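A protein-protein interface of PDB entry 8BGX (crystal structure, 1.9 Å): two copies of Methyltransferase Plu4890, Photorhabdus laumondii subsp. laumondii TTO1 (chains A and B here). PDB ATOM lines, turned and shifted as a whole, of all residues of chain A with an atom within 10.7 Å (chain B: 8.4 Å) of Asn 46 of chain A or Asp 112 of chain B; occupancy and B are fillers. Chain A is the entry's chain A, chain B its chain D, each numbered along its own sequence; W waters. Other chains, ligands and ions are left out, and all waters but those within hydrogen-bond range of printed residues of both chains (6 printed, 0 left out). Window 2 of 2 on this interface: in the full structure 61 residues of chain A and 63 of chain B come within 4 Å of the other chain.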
ATOM      1  N   THR A  22     -17.656  -7.532 -23.323  1.00  0.00           N
ATOM      2  CA  THR A  22     -17.687  -8.907 -22.742  1.00  0.00           C
ATOM      3  C   THR A  22     -18.340  -8.893 -21.354  1.00  0.00           C
ATOM      4  O   THR A  22     -18.713  -9.978 -20.868  1.00  0.00           O
ATOM      5  CB  THR A  22     -16.285  -9.511 -22.599  1.00  0.00           C
ATOM      6  OG1 THR A  22     -15.509  -8.625 -21.787  1.00  0.00           O
ATOM      7  CG2 THR A  22     -15.611  -9.752 -23.931  1.00  0.00           C
ATOM      8  N   LEU A  24     -16.622  -7.952 -18.664  1.00  0.00           N
ATOM      9  CA  LEU A  24     -15.504  -8.107 -17.691  1.00  0.00           C
ATOM     10  C   LEU A  24     -15.428  -6.855 -16.806  1.00  0.00           C
ATOM     11  O   LEU A  24     -15.201  -7.003 -15.595  1.00  0.00           O
ATOM     12  CB  LEU A  24     -14.185  -8.358 -18.431  1.00  0.00           C
ATOM     13  CG  LEU A  24     -14.005  -9.771 -18.986  1.00  0.00           C
ATOM     14  CD1 LEU A  24     -12.838  -9.831 -19.962  1.00  0.00           C
ATOM     15  CD2 LEU A  24     -13.810 -10.779 -17.862  1.00  0.00           C
ATOM     16  N   ASP A  35      -8.625  -8.987  -7.973  1.00  0.00           N
ATOM     17  CA  ASP A  35      -7.558  -9.992  -8.199  1.00  0.00           C
ATOM     18  C   ASP A  35      -7.883 -10.722  -9.506  1.00  0.00           C
ATOM     19  O   ASP A  35      -8.966 -11.333  -9.583  1.00  0.00           O
ATOM     20  CB  ASP A  35      -7.445 -10.962  -7.023  1.00  0.00           C
ATOM     21  CG  ASP A  35      -6.380 -12.018  -7.239  1.00  0.00           C
ATOM     22  OD1 ASP A  35      -6.741 -13.118  -7.685  1.00  0.00           O
ATOM     23  OD2 ASP A  35      -5.202 -11.723  -6.967  1.00  0.00           O
ATOM     24  N   ILE A  36      -6.982 -10.657 -10.488  1.00  0.00           N
ATOM     25  CA  ILE A  36      -7.210 -11.215 -11.854  1.00  0.00           C
ATOM     26  C   ILE A  36      -7.210 -12.748 -11.787  1.00  0.00           C
ATOM     27  O   ILE A  36      -7.940 -13.358 -12.580  1.00  0.00           O
ATOM     28  CB  ILE A  36      -6.183 -10.669 -12.867  1.00  0.00           C
ATOM     29  CG1 ILE A  36      -6.201  -9.137 -12.925  1.00  0.00           C
ATOM     30  CG2 ILE A  36      -6.397 -11.284 -14.242  1.00  0.00           C
ATOM     31  CD1 ILE A  36      -7.569  -8.523 -13.194  1.00  0.00           C
ATOM     32  N   SER A  37      -6.435 -13.355 -10.881  1.00  0.00           N
ATOM     33  CA  SER A  37      -6.450 -14.829 -10.664  1.00  0.00           C
ATOM     34  C   SER A  37      -7.876 -15.271 -10.298  1.00  0.00           C
ATOM     35  O   SER A  37      -8.362 -16.250 -10.897  1.00  0.00           O
ATOM     36  CB  SER A  37      -5.441 -15.264  -9.627  1.00  0.00           C
ATOM     37  OG  SER A  37      -4.118 -15.143 -10.130  1.00  0.00           O
ATOM     38  N   GLU A  38      -8.527 -14.561  -9.369  1.00  0.00           N
ATOM     39  CA  GLU A  38      -9.899 -14.877  -8.887  1.00  0.00           C
ATOM     40  C   GLU A  38     -10.909 -14.606 -10.009  1.00  0.00           C
ATOM     41  O   GLU A  38     -11.788 -15.454 -10.220  1.00  0.00           O
ATOM     42  CB  GLU A  38     -10.230 -14.086  -7.617  1.00  0.00           C
ATOM     43  CG  GLU A  38     -11.592 -14.416  -7.015  1.00  0.00           C
ATOM     44  CD  GLU A  38     -11.852 -15.877  -6.666  1.00  0.00           C
ATOM     45  OE1 GLU A  38     -10.914 -16.562  -6.198  1.00  0.00           O
ATOM     46  OE2 GLU A  38     -12.999 -16.329  -6.852  1.00  0.00           O
ATOM     47  N   LEU A  39     -10.781 -13.480 -10.716  1.00  0.00           N
ATOM     48  CA  LEU A  39     -11.687 -13.124 -11.842  1.00  0.00           C
ATOM     49  C   LEU A  39     -11.610 -14.216 -12.920  1.00  0.00           C
ATOM     50  O   LEU A  39     -12.671 -14.614 -13.449  1.00  0.00           O
ATOM     51  CB  LEU A  39     -11.304 -11.750 -12.405  1.00  0.00           C
ATOM     52  CG  LEU A  39     -12.139 -11.271 -13.593  1.00  0.00           C
ATOM     53  CD1 LEU A  39     -13.613 -11.166 -13.225  1.00  0.00           C
ATOM     54  CD2 LEU A  39     -11.623  -9.936 -14.106  1.00  0.00           C
ATOM     55  N   SER A  40     -10.397 -14.687 -13.231  1.00  0.00           N
ATOM     56  CA  SER A  40     -10.142 -15.744 -14.244  1.00  0.00           C
ATOM     57  C   SER A  40     -10.839 -17.047 -13.836  1.00  0.00           C
ATOM     58  O   SER A  40     -11.487 -17.659 -14.706  1.00  0.00           O
ATOM     59  CB  SER A  40      -8.669 -15.953 -14.461  1.00  0.00           C
ATOM     60  OG  SER A  40      -8.104 -14.837 -15.130  1.00  0.00           O
ATOM     61  N   ARG A  41     -10.718 -17.448 -12.568  1.00  0.00           N
ATOM     62  CA  ARG A  41     -11.371 -18.680 -12.046  1.00  0.00           C
ATOM     63  C   ARG A  41     -12.896 -18.530 -12.130  1.00  0.00           C
ATOM     64  O   ARG A  41     -13.550 -19.483 -12.577  1.00  0.00           O
ATOM     65  CB  ARG A  41     -10.923 -18.980 -10.612  1.00  0.00           C
ATOM     66  CG  ARG A  41      -9.486 -19.470 -10.503  1.00  0.00           C
ATOM     67  CD  ARG A  41      -9.167 -19.927  -9.094  1.00  0.00           C
ATOM     68  NE  ARG A  41      -9.232 -18.828  -8.135  1.00  0.00           N
ATOM     69  CZ  ARG A  41      -8.197 -18.104  -7.716  1.00  0.00           C
ATOM     70  NH1 ARG A  41      -8.393 -17.140  -6.832  1.00  0.00           N
ATOM     71  NH2 ARG A  41      -6.972 -18.342  -8.163  1.00  0.00           N
ATOM     72  N   LYS A  42     -13.432 -17.370 -11.742  1.00  0.00           N
ATOM     73  CA  LYS A  42     -14.898 -17.118 -11.649  1.00  0.00           C
ATOM     74  C   LYS A  42     -15.520 -16.977 -13.049  1.00  0.00           C
ATOM     75  O   LYS A  42     -16.586 -17.584 -13.277  1.00  0.00           O
ATOM     76  CB  LYS A  42     -15.171 -15.869 -10.802  1.00  0.00           C
ATOM     77  CG  LYS A  42     -16.595 -15.337 -10.887  1.00  0.00           C
ATOM     78  CD  LYS A  42     -16.999 -14.452  -9.730  1.00  0.00           C
ATOM     79  CE  LYS A  42     -18.439 -13.994  -9.838  1.00  0.00           C
ATOM     80  NZ  LYS A  42     -18.889 -13.292  -8.613  1.00  0.00           N
ATOM     81  N   SER A  43     -14.900 -16.199 -13.940  1.00  0.00           N
ATOM     82  CA  SER A  43     -15.470 -15.793 -15.256  1.00  0.00           C
ATOM     83  C   SER A  43     -15.034 -16.742 -16.379  1.00  0.00           C
ATOM     84  O   SER A  43     -15.731 -16.773 -17.412  1.00  0.00           O
ATOM     85  CB  SER A  43     -15.087 -14.381 -15.586  1.00  0.00           C
ATOM     86  OG  SER A  43     -13.689 -14.281 -15.821  1.00  0.00           O
ATOM     87  N   GLY A  44     -13.907 -17.440 -16.209  1.00  0.00           N
ATOM     88  CA  GLY A  44     -13.331 -18.332 -17.235  1.00  0.00           C
ATOM     89  C   GLY A  44     -12.507 -17.572 -18.263  1.00  0.00           C
ATOM     90  O   GLY A  44     -12.157 -18.177 -19.299  1.00  0.00           O
ATOM     91  N   VAL A  45     -12.197 -16.296 -18.013  1.00  0.00           N
ATOM     92  CA  VAL A  45     -11.280 -15.503 -18.883  1.00  0.00           C
ATOM     93  C   VAL A  45      -9.868 -16.065 -18.683  1.00  0.00           C
ATOM     94  O   VAL A  45      -9.538 -16.442 -17.545  1.00  0.00           O
ATOM     95  CB  VAL A  45     -11.367 -13.987 -18.608  1.00  0.00           C
ATOM     96  CG1 VAL A  45     -10.687 -13.571 -17.313  1.00  0.00           C
ATOM     97  CG2 VAL A  45     -10.827 -13.174 -19.772  1.00  0.00           C
ATOM     98  N   ASN A  46      -9.089 -16.168 -19.760  1.00  0.00           N
ATOM     99  CA  ASN A  46      -7.691 -16.665 -19.725  1.00  0.00           C
ATOM    100  C   ASN A  46      -6.850 -15.699 -18.885  1.00  0.00           C
ATOM    101  O   ASN A  46      -6.782 -14.515 -19.257  1.00  0.00           O
ATOM    102  CB  ASN A  46      -7.116 -16.823 -21.131  1.00  0.00           C
ATOM    103  CG  ASN A  46      -5.738 -17.443 -21.113  1.00  0.00           C
ATOM    104  OD1 ASN A  46      -4.738 -16.734 -21.083  1.00  0.00           O
ATOM    105  ND2 ASN A  46      -5.681 -18.761 -21.081  1.00  0.00           N
ATOM    106  N   TYR A  47      -6.242 -16.182 -17.794  1.00  0.00           N
ATOM    107  CA  TYR A  47      -5.510 -15.345 -16.807  1.00  0.00           C
ATOM    108  C   TYR A  47      -4.369 -14.571 -17.481  1.00  0.00           C
ATOM    109  O   TYR A  47      -4.310 -13.340 -17.313  1.00  0.00           O
ATOM    110  CB  TYR A  47      -4.935 -16.171 -15.654  1.00  0.00           C
ATOM    111  CG  TYR A  47      -3.991 -15.368 -14.797  1.00  0.00           C
ATOM    112  CD1 TYR A  47      -4.472 -14.500 -13.829  1.00  0.00           C
ATOM    113  CD2 TYR A  47      -2.621 -15.409 -15.009  1.00  0.00           C
ATOM    114  CE1 TYR A  47      -3.615 -13.727 -13.062  1.00  0.00           C
ATOM    115  CE2 TYR A  47      -1.752 -14.646 -14.249  1.00  0.00           C
ATOM    116  CZ  TYR A  47      -2.249 -13.802 -13.271  1.00  0.00           C
ATOM    117  OH  TYR A  47      -1.396 -13.048 -12.519  1.00  0.00           O
ATOM    118  N   ALA A  48      -3.472 -15.271 -18.181  1.00  0.00           N
ATOM    119  CA  ALA A  48      -2.223 -14.704 -18.742  1.00  0.00           C
ATOM    120  C   ALA A  48      -2.572 -13.638 -19.788  1.00  0.00           C
ATOM    121  O   ALA A  48      -1.970 -12.552 -19.761  1.00  0.00           O
ATOM    122  CB  ALA A  48      -1.358 -15.797 -19.326  1.00  0.00           C
ATOM    123  N   ARG A  49      -3.535 -13.935 -20.660  1.00  0.00           N
ATOM    124  CA  ARG A  49      -3.909 -13.053 -21.796  1.00  0.00           C
ATOM    125  C   ARG A  49      -4.715 -11.855 -21.279  1.00  0.00           C
ATOM    126  O   ARG A  49      -4.522 -10.745 -21.817  1.00  0.00           O
ATOM    127  CB  ARG A  49      -4.655 -13.861 -22.856  1.00  0.00           C
ATOM    128  CG  ARG A  49      -3.776 -14.887 -23.560  1.00  0.00           C
ATOM    129  CD  ARG A  49      -4.590 -15.762 -24.482  1.00  0.00           C
ATOM    130  NE  ARG A  49      -5.289 -14.929 -25.451  1.00  0.00           N
ATOM    131  CZ  ARG A  49      -6.543 -15.099 -25.852  1.00  0.00           C
ATOM    132  NH1 ARG A  49      -7.277 -16.089 -25.373  1.00  0.00           N
ATOM    133  NH2 ARG A  49      -7.063 -14.261 -26.733  1.00  0.00           N
ATOM    134  N   PHE A  50      -5.571 -12.044 -20.272  1.00  0.00           N
ATOM    135  CA  PHE A  50      -6.351 -10.927 -19.677  1.00  0.00           C
ATOM    136  C   PHE A  50      -5.413 -10.009 -18.883  1.00  0.00           C
ATOM    137  O   PHE A  50      -5.606  -8.778 -18.928  1.00  0.00           O
ATOM    138  CB  PHE A  50      -7.521 -11.409 -18.818  1.00  0.00           C
ATOM    139  CG  PHE A  50      -8.399 -10.272 -18.359  1.00  0.00           C
ATOM    140  CD1 PHE A  50      -8.989  -9.423 -19.285  1.00  0.00           C
ATOM    141  CD2 PHE A  50      -8.602 -10.020 -17.014  1.00  0.00           C
ATOM    142  CE1 PHE A  50      -9.777  -8.358 -18.875  1.00  0.00           C
ATOM    143  CE2 PHE A  50      -9.394  -8.956 -16.604  1.00  0.00           C
ATOM    144  CZ  PHE A  50      -9.982  -8.130 -17.535  1.00  0.00           C
ATOM    145  N   SER A  51      -4.415 -10.579 -18.201  1.00  0.00           N
ATOM    146  CA  SER A  51      -3.402  -9.811 -17.428  1.00  0.00           C
ATOM    147  C   SER A  51      -2.664  -8.851 -18.365  1.00  0.00           C
ATOM    148  O   SER A  51      -2.419  -7.701 -17.954  1.00  0.00           O
ATOM    149  CB  SER A  51      -2.449 -10.717 -16.694  1.00  0.00           C
ATOM    150  OG  SER A  51      -3.081 -11.265 -15.552  1.00  0.00           O
ATOM    151  N   ARG A  52      -2.337  -9.307 -19.577  1.00  0.00           N
ATOM    152  CA  ARG A  52      -1.672  -8.486 -20.621  1.00  0.00           C
ATOM    153  C   ARG A  52      -2.607  -7.340 -21.030  1.00  0.00           C
ATOM    154  O   ARG A  52      -2.120  -6.199 -21.133  1.00  0.00           O
ATOM    155  CB  ARG A  52      -1.248  -9.366 -21.797  1.00  0.00           C
ATOM    156  CG  ARG A  52       0.003 -10.188 -21.515  1.00  0.00           C
ATOM    157  CD  ARG A  52       0.137 -11.365 -22.458  1.00  0.00           C
ATOM    158  NE  ARG A  52       0.182 -10.950 -23.853  1.00  0.00           N
ATOM    159  CZ  ARG A  52       0.008 -11.754 -24.898  1.00  0.00           C
ATOM    160  NH1 ARG A  52      -0.227 -13.044 -24.728  1.00  0.00           N
ATOM    161  NH2 ARG A  52       0.071 -11.259 -26.120  1.00  0.00           N
ATOM    162  N   LEU A  53      -3.902  -7.619 -21.217  1.00  0.00           N
ATOM    163  CA  LEU A  53      -4.921  -6.577 -21.517  1.00  0.00           C
ATOM    164  C   LEU A  53      -4.937  -5.555 -20.374  1.00  0.00           C
ATOM    165  O   LEU A  53      -4.865  -4.359 -20.668  1.00  0.00           O
ATOM    166  CB  LEU A  53      -6.304  -7.208 -21.720  1.00  0.00           C
ATOM    167  CG  LEU A  53      -7.441  -6.224 -22.018  1.00  0.00           C
ATOM    168  CD1 LEU A  53      -7.081  -5.273 -23.151  1.00  0.00           C
ATOM    169  CD2 LEU A  53      -8.724  -6.966 -22.355  1.00  0.00           C
ATOM    170  N   CYS A  54      -4.988  -6.016 -19.122  1.00  0.00           N
ATOM    171  CA  CYS A  54      -5.016  -5.150 -17.909  1.00  0.00           C
ATOM    172  C   CYS A  54      -3.806  -4.202 -17.904  1.00  0.00           C
ATOM    173  O   CYS A  54      -4.000  -3.021 -17.576  1.00  0.00           O
ATOM    174  CB  CYS A  54      -5.092  -5.977 -16.630  1.00  0.00           C
ATOM    175  SG  CYS A  54      -6.729  -6.709 -16.365  1.00  0.00           S
ATOM    176  N   GLY B 106     -12.424  -9.916 -27.444  1.00  0.00           N
ATOM    177  CA  GLY B 106     -13.167 -10.143 -26.190  1.00  0.00           C
ATOM    178  C   GLY B 106     -13.584 -11.596 -26.037  1.00  0.00           C
ATOM    179  O   GLY B 106     -13.342 -12.168 -24.956  1.00  0.00           O
ATOM    180  N   LYS B 107     -14.186 -12.177 -27.080  1.00  0.00           N
ATOM    181  CA  LYS B 107     -14.662 -13.587 -27.091  1.00  0.00           C
ATOM    182  C   LYS B 107     -13.461 -14.541 -27.057  1.00  0.00           C
ATOM    183  O   LYS B 107     -13.570 -15.587 -26.390  1.00  0.00           O
ATOM    184  CB  LYS B 107     -15.558 -13.845 -28.304  1.00  0.00           C
ATOM    185  CG  LYS B 107     -16.927 -13.181 -28.226  1.00  0.00           C
ATOM    186  CD  LYS B 107     -17.659 -13.128 -29.549  1.00  0.00           C
ATOM    187  CE  LYS B 107     -18.736 -12.065 -29.586  1.00  0.00           C
ATOM    188  NZ  LYS B 107     -19.583 -12.188 -30.794  1.00  0.00           N
ATOM    189  N   SER B 108     -12.360 -14.194 -27.733  1.00  0.00           N
ATOM    190  CA  SER B 108     -11.132 -15.031 -27.810  1.00  0.00           C
ATOM    191  C   SER B 108     -10.563 -15.281 -26.405  1.00  0.00           C
ATOM    192  O   SER B 108      -9.967 -16.345 -26.208  1.00  0.00           O
ATOM    193  CB  SER B 108     -10.094 -14.431 -28.733  1.00  0.00           C
ATOM    194  OG  SER B 108      -9.400 -13.359 -28.109  1.00  0.00           O
ATOM    195  N   LEU B 109     -10.763 -14.344 -25.468  1.00  0.00           N
ATOM    196  CA  LEU B 109     -10.205 -14.387 -24.089  1.00  0.00           C
ATOM    197  C   LEU B 109     -10.902 -15.465 -23.242  1.00  0.00           C
ATOM    198  O   LEU B 109     -10.326 -15.836 -22.200  1.00  0.00           O
ATOM    199  CB  LEU B 109     -10.349 -13.008 -23.435  1.00  0.00           C
ATOM    200  CG  LEU B 109      -9.454 -11.904 -23.996  1.00  0.00           C
ATOM    201  CD1 LEU B 109      -9.886 -10.545 -23.467  1.00  0.00           C
ATOM    202  CD2 LEU B 109      -7.985 -12.155 -23.671  1.00  0.00           C
ATOM    203  N   PHE B 110     -12.088 -15.931 -23.650  1.00  0.00           N
ATOM    204  CA  PHE B 110     -12.901 -16.937 -22.915  1.00  0.00           C
ATOM    205  C   PHE B 110     -12.734 -18.335 -23.527  1.00  0.00           C
ATOM    206  O   PHE B 110     -13.360 -19.276 -23.002  1.00  0.00           O
ATOM    207  CB  PHE B 110     -14.371 -16.510 -22.886  1.00  0.00           C
ATOM    208  CG  PHE B 110     -14.632 -15.321 -21.999  1.00  0.00           C
ATOM    209  CD1 PHE B 110     -14.965 -15.489 -20.663  1.00  0.00           C
ATOM    210  CD2 PHE B 110     -14.509 -14.031 -22.493  1.00  0.00           C
ATOM    211  CE1 PHE B 110     -15.191 -14.392 -19.846  1.00  0.00           C
ATOM    212  CE2 PHE B 110     -14.735 -12.935 -21.674  1.00  0.00           C
ATOM    213  CZ  PHE B 110     -15.077 -13.117 -20.355  1.00  0.00           C
ATOM    214  N   GLU B 111     -11.919 -18.471 -24.578  1.00  0.00           N
ATOM    215  CA  GLU B 111     -11.648 -19.759 -25.276  1.00  0.00           C
ATOM    216  C   GLU B 111     -10.215 -20.206 -24.964  1.00  0.00           C
ATOM    217  O   GLU B 111      -9.352 -19.328 -24.767  1.00  0.00           O
ATOM    218  CB  GLU B 111     -11.841 -19.614 -26.788  1.00  0.00           C
ATOM    219  CG  GLU B 111     -13.214 -19.103 -27.192  1.00  0.00           C
ATOM    220  CD  GLU B 111     -14.388 -19.988 -26.806  1.00  0.00           C
ATOM    221  OE1 GLU B 111     -15.515 -19.458 -26.707  1.00  0.00           O
ATOM    222  OE2 GLU B 111     -14.179 -21.202 -26.614  1.00  0.00           O
ATOM    223  N   ASP B 112      -9.980 -21.520 -24.920  1.00  0.00           N
ATOM    224  CA  ASP B 112      -8.636 -22.126 -24.714  1.00  0.00           C
ATOM    225  C   ASP B 112      -8.424 -23.217 -25.774  1.00  0.00           C
ATOM    226  O   ASP B 112      -7.800 -24.241 -25.456  1.00  0.00           O
ATOM    227  CB  ASP B 112      -8.490 -22.637 -23.276  1.00  0.00           C
ATOM    228  CG  ASP B 112      -7.068 -22.583 -22.737  1.00  0.00           C
ATOM    229  OD1 ASP B 112      -6.812 -23.227 -21.699  1.00  0.00           O
ATOM    230  OD2 ASP B 112      -6.228 -21.890 -23.352  1.00  0.00           O
ATOM    231  N   ASP B 113      -8.896 -22.965 -27.000  1.00  0.00           N
ATOM    232  CA  ASP B 113      -8.898 -23.916 -28.145  1.00  0.00           C
ATOM    233  C   ASP B 113      -7.688 -23.647 -29.053  1.00  0.00           C
ATOM    234  O   ASP B 113      -7.553 -24.348 -30.074  1.00  0.00           O
ATOM    235  CB  ASP B 113     -10.215 -23.822 -28.926  1.00  0.00           C
ATOM    236  CG  ASP B 113     -10.621 -22.410 -29.336  1.00  0.00           C
ATOM    237  OD1 ASP B 113      -9.863 -21.456 -29.030  1.00  0.00           O
ATOM    238  OD2 ASP B 113     -11.701 -22.268 -29.950  1.00  0.00           O
ATOM    239  N   GLY B 114      -6.851 -22.665 -28.701  1.00  0.00           N
ATOM    240  CA  GLY B 114      -5.695 -22.226 -29.507  1.00  0.00           C
ATOM    241  C   GLY B 114      -6.123 -21.505 -30.779  1.00  0.00           C
ATOM    242  O   GLY B 114      -5.335 -21.497 -31.741  1.00  0.00           O
ATOM    243  N   LYS B 115      -7.321 -20.910 -30.800  1.00  0.00           N
ATOM    244  CA  LYS B 115      -7.825 -20.145 -31.973  1.00  0.00           C
ATOM    245  C   LYS B 115      -7.724 -18.646 -31.673  1.00  0.00           C
ATOM    246  O   LYS B 115      -8.385 -18.174 -30.724  1.00  0.00           O
ATOM    247  CB  LYS B 115      -9.243 -20.592 -32.344  1.00  0.00           C
ATOM    248  CG  LYS B 115      -9.318 -22.007 -32.903  1.00  0.00           C
ATOM    249  CD  LYS B 115     -10.593 -22.328 -33.648  1.00  0.00           C
ATOM    250  CE  LYS B 115     -10.616 -23.752 -34.167  1.00  0.00           C
ATOM    251  NZ  LYS B 115     -11.816 -24.020 -34.995  1.00  0.00           N
ATOM    252  N   MET B 120     -11.018 -16.884 -35.376  1.00  0.00           N
ATOM    253  CA  MET B 120     -12.456 -16.872 -34.986  1.00  0.00           C
ATOM    254  C   MET B 120     -13.255 -16.023 -35.989  1.00  0.00           C
ATOM    255  O   MET B 120     -14.388 -16.416 -36.319  1.00  0.00           O
ATOM    256  CB  MET B 120     -12.641 -16.341 -33.560  1.00  0.00           C
ATOM    257  CG  MET B 120     -12.149 -17.316 -32.504  1.00  0.00           C
ATOM    258  SD  MET B 120     -12.166 -16.640 -30.824  1.00  0.00           S
ATOM    259  CE  MET B 120     -13.921 -16.671 -30.471  1.00  0.00           C
ATOM    260  N   ASP B 274      -1.511 -10.882 -29.798  1.00  0.00           N
ATOM    261  CA  ASP B 274      -2.513 -11.794 -29.190  1.00  0.00           C
ATOM    262  C   ASP B 274      -3.694 -11.966 -30.159  1.00  0.00           C
ATOM    263  O   ASP B 274      -4.050 -13.123 -30.469  1.00  0.00           O
ATOM    264  CB  ASP B 274      -2.960 -11.290 -27.817  1.00  0.00           C
ATOM    265  CG  ASP B 274      -3.794 -12.298 -27.050  1.00  0.00           C
ATOM    266  OD1 ASP B 274      -3.449 -13.488 -27.088  1.00  0.00           O
ATOM    267  OD2 ASP B 274      -4.795 -11.888 -26.438  1.00  0.00           O
ATOM    268  N   LEU B 278      -2.274 -15.271 -31.376  1.00  0.00           N
ATOM    269  CA  LEU B 278      -2.020 -15.729 -29.979  1.00  0.00           C
ATOM    270  C   LEU B 278      -0.509 -15.665 -29.712  1.00  0.00           C
ATOM    271  O   LEU B 278       0.018 -16.531 -28.981  1.00  0.00           O
ATOM    272  CB  LEU B 278      -2.569 -17.144 -29.758  1.00  0.00           C
ATOM    273  CG  LEU B 278      -4.092 -17.260 -29.702  1.00  0.00           C
ATOM    274  CD1 LEU B 278      -4.524 -18.716 -29.677  1.00  0.00           C
ATOM    275  CD2 LEU B 278      -4.655 -16.525 -28.494  1.00  0.00           C
HETATM  276  O   HOH W   1      -6.658 -13.819 -29.971  1.00  0.00           O
HETATM  277  O   HOH W   2      -1.239 -14.606 -26.676  1.00  0.00           O
HETATM  278  O   HOH W   3      -4.495 -10.126 -24.554  1.00  0.00           O
HETATM  279  O   HOH W   4      -6.728 -18.604 -24.198  1.00  0.00           O
HETATM  280  O   HOH W   5     -14.204 -19.880 -20.766  1.00  0.00           O
HETATM  281  O   HOH W   6     -10.315 -18.962 -21.136  1.00  0.00           O
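Water W5 bridges the backbone carbonyl oxygen of Phe 110 of chain B (2.5 Å) and the backbone carbonyl oxygen of Gly 44 of chain A (3.0 Å).
Water W2 lies within hydrogen-bond range of OD1 of Asp 274 of chain B (2.5 Å), NH1 of Arg 52 of chain A (2.7 Å) and O of Leu 278 of chain B (3.3 Å).
Water W3 lies within hydrogen-bond range of OD2 of Asp 274 of chain B and O of Arg 49 of chain A.
Water W6 lies within hydrogen-bond range of the backbone carbonyl oxygen of Gly 44 of chain A (2.7 Å), the backbone carbonyl oxygen of Leu 109 of chain B (3.3 Å) and the backbone NH of Asn 46 of chain A (3.3 Å).
Water W1 lies within hydrogen-bond range of the backbone carbonyl oxygen (O) of Asp 274 of chain B (2.7 Å), the guanidinium group (NH2) of Arg 49 of chain A (3.3 Å) and the side-chain hydroxyl (OG) of Ser 108 of chain B (3.3 Å).
Water W4 lies within hydrogen-bond range of the backbone carbonyl oxygen (O) of Glu 111 of chain B, the guanidinium group (NH1) of Arg 49 of chain A, the side-chain amide nitrogen (ND2) of Asn 46 of chain A and the side-chain carboxylate (OD2) of Asp 112 of chain B.
N of Arg 49 of chain A sits at hydrogen-bond distance from OD1 of Asn 46 of chain A (3.1 Å).
The backbone carbonyl oxygen (O) of Val 45 of chain A is in hydrogen-bond range of the side-chain hydroxyl (OG) of Ser 40 of chain A.
The backbone carbonyl oxygen (O) of Leu 39 of chain A is in hydrogen-bond range of the side-chain hydroxyl (OG) of Ser 43 of chain A, at 2.6 Å.
The backbone NH of Ala 48 of chain A lies close to the side-chain amide oxygen of Asn 46 of chain A, at 3.5 Å.
The backbone NH of Val 45 of chain A lies close to the side-chain hydroxyl of Ser 43 of chain A (3.3 Å).
The side-chain hydroxyl of Thr 22 of chain A sits close to the backbone NH of Leu 24 of chain A, at 3.4 Å.
No position is printed for both chains.
Of the 16 pairs that touch across the chains among the printed residues, none has its exchanged pair printed and touching as well.
Ser 40 of chain A touches none of the printed residues of chain B.
Printed residues of chain B within 4 Å of Gly 44 of chain A: Phe 110 (3.9 Å).
Val 45 of chain A touches just these residues of chain B: Leu 109 (3.5 Å) and Phe 110 (3.9 Å).
Of chain B, only Leu 109 (2.8 Å) and Asp 112 (3.9 Å) come within 4 Å of Asn 46 of chain A.
Of the printed residues of chain B, Leu 53 of chain A touches Leu 109 (3.9 Å).
Of chain A, only Val 45 (3.5 Å), Asn 46 (2.8 Å), Arg 49 (3.6 Å) and Leu 53 (3.9 Å) come within 4 Å of Leu 109 of chain B.
Of chain A, only Arg 49 (3.9 Å) comes within 4 Å of Glu 111 of chain B.
No residue of chain A comes within 4 Å of Asp 113 of chain B.
Met 120 of chain B touches none of the printed residues of chain A.
The nearest residue of chain B that does not touch Asn 46 of chain A is Phe 110 of chain B (4.9 Å).
OD1 of Asp 274 of chain B is in salt-bridge range of NE of Arg 49 of chain A, at 2.9 Å.
O of Ser 108 of chain B lies within hydrogen-bond range of NH1 of Arg 49 of chain A, 2.8 Å away.
N of Asn 46 of chain A sits at hydrogen-bond distance from O of Leu 109 of chain B, 2.8 Å away.
Among the printed residues, merely in contact across the chains: Thr 22 of chain A with Gly 106 of chain B (3.4 Å), Ser 43 of chain A with Phe 110 of chain B (3.4 Å), Val 45 of chain A with Leu 109 of chain B (3.5 Å), Arg 52 of chain A with Asp 274 of chain B (3.5 Å), Arg 49 of chain A with Leu 278 of chain B (3.5 Å), Arg 49 of chain A with Leu 109 of chain B (3.6 Å), Leu 24 of chain A with Phe 110 of chain B (3.6 Å), Thr 22 of chain A with Phe 110 of chain B (3.9 Å), Arg 49 of chain A with Glu 111 of chain B (3.9 Å), Gly 44 of chain A with Phe 110 of chain B (3.9 Å), Asn 46 of chain A with Asp 112 of chain B (3.9 Å), Val 45 of chain A with Phe 110 of chain B (3.9 Å) and Leu 53 of chain A with Leu 109 of chain B (3.9 Å).
Of the 13 printed residues of chain B, 8 touch a printed residue of chain A.
Hydrophobic or aromatic side chains of chain B within 4 Å of the printed part of chain A: Leu 109, Phe 110 and Leu 278.
Hydrophobic or aromatic side chains of chain A that line the printed part of chain B: Leu 24, Val 45 and Leu 53.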
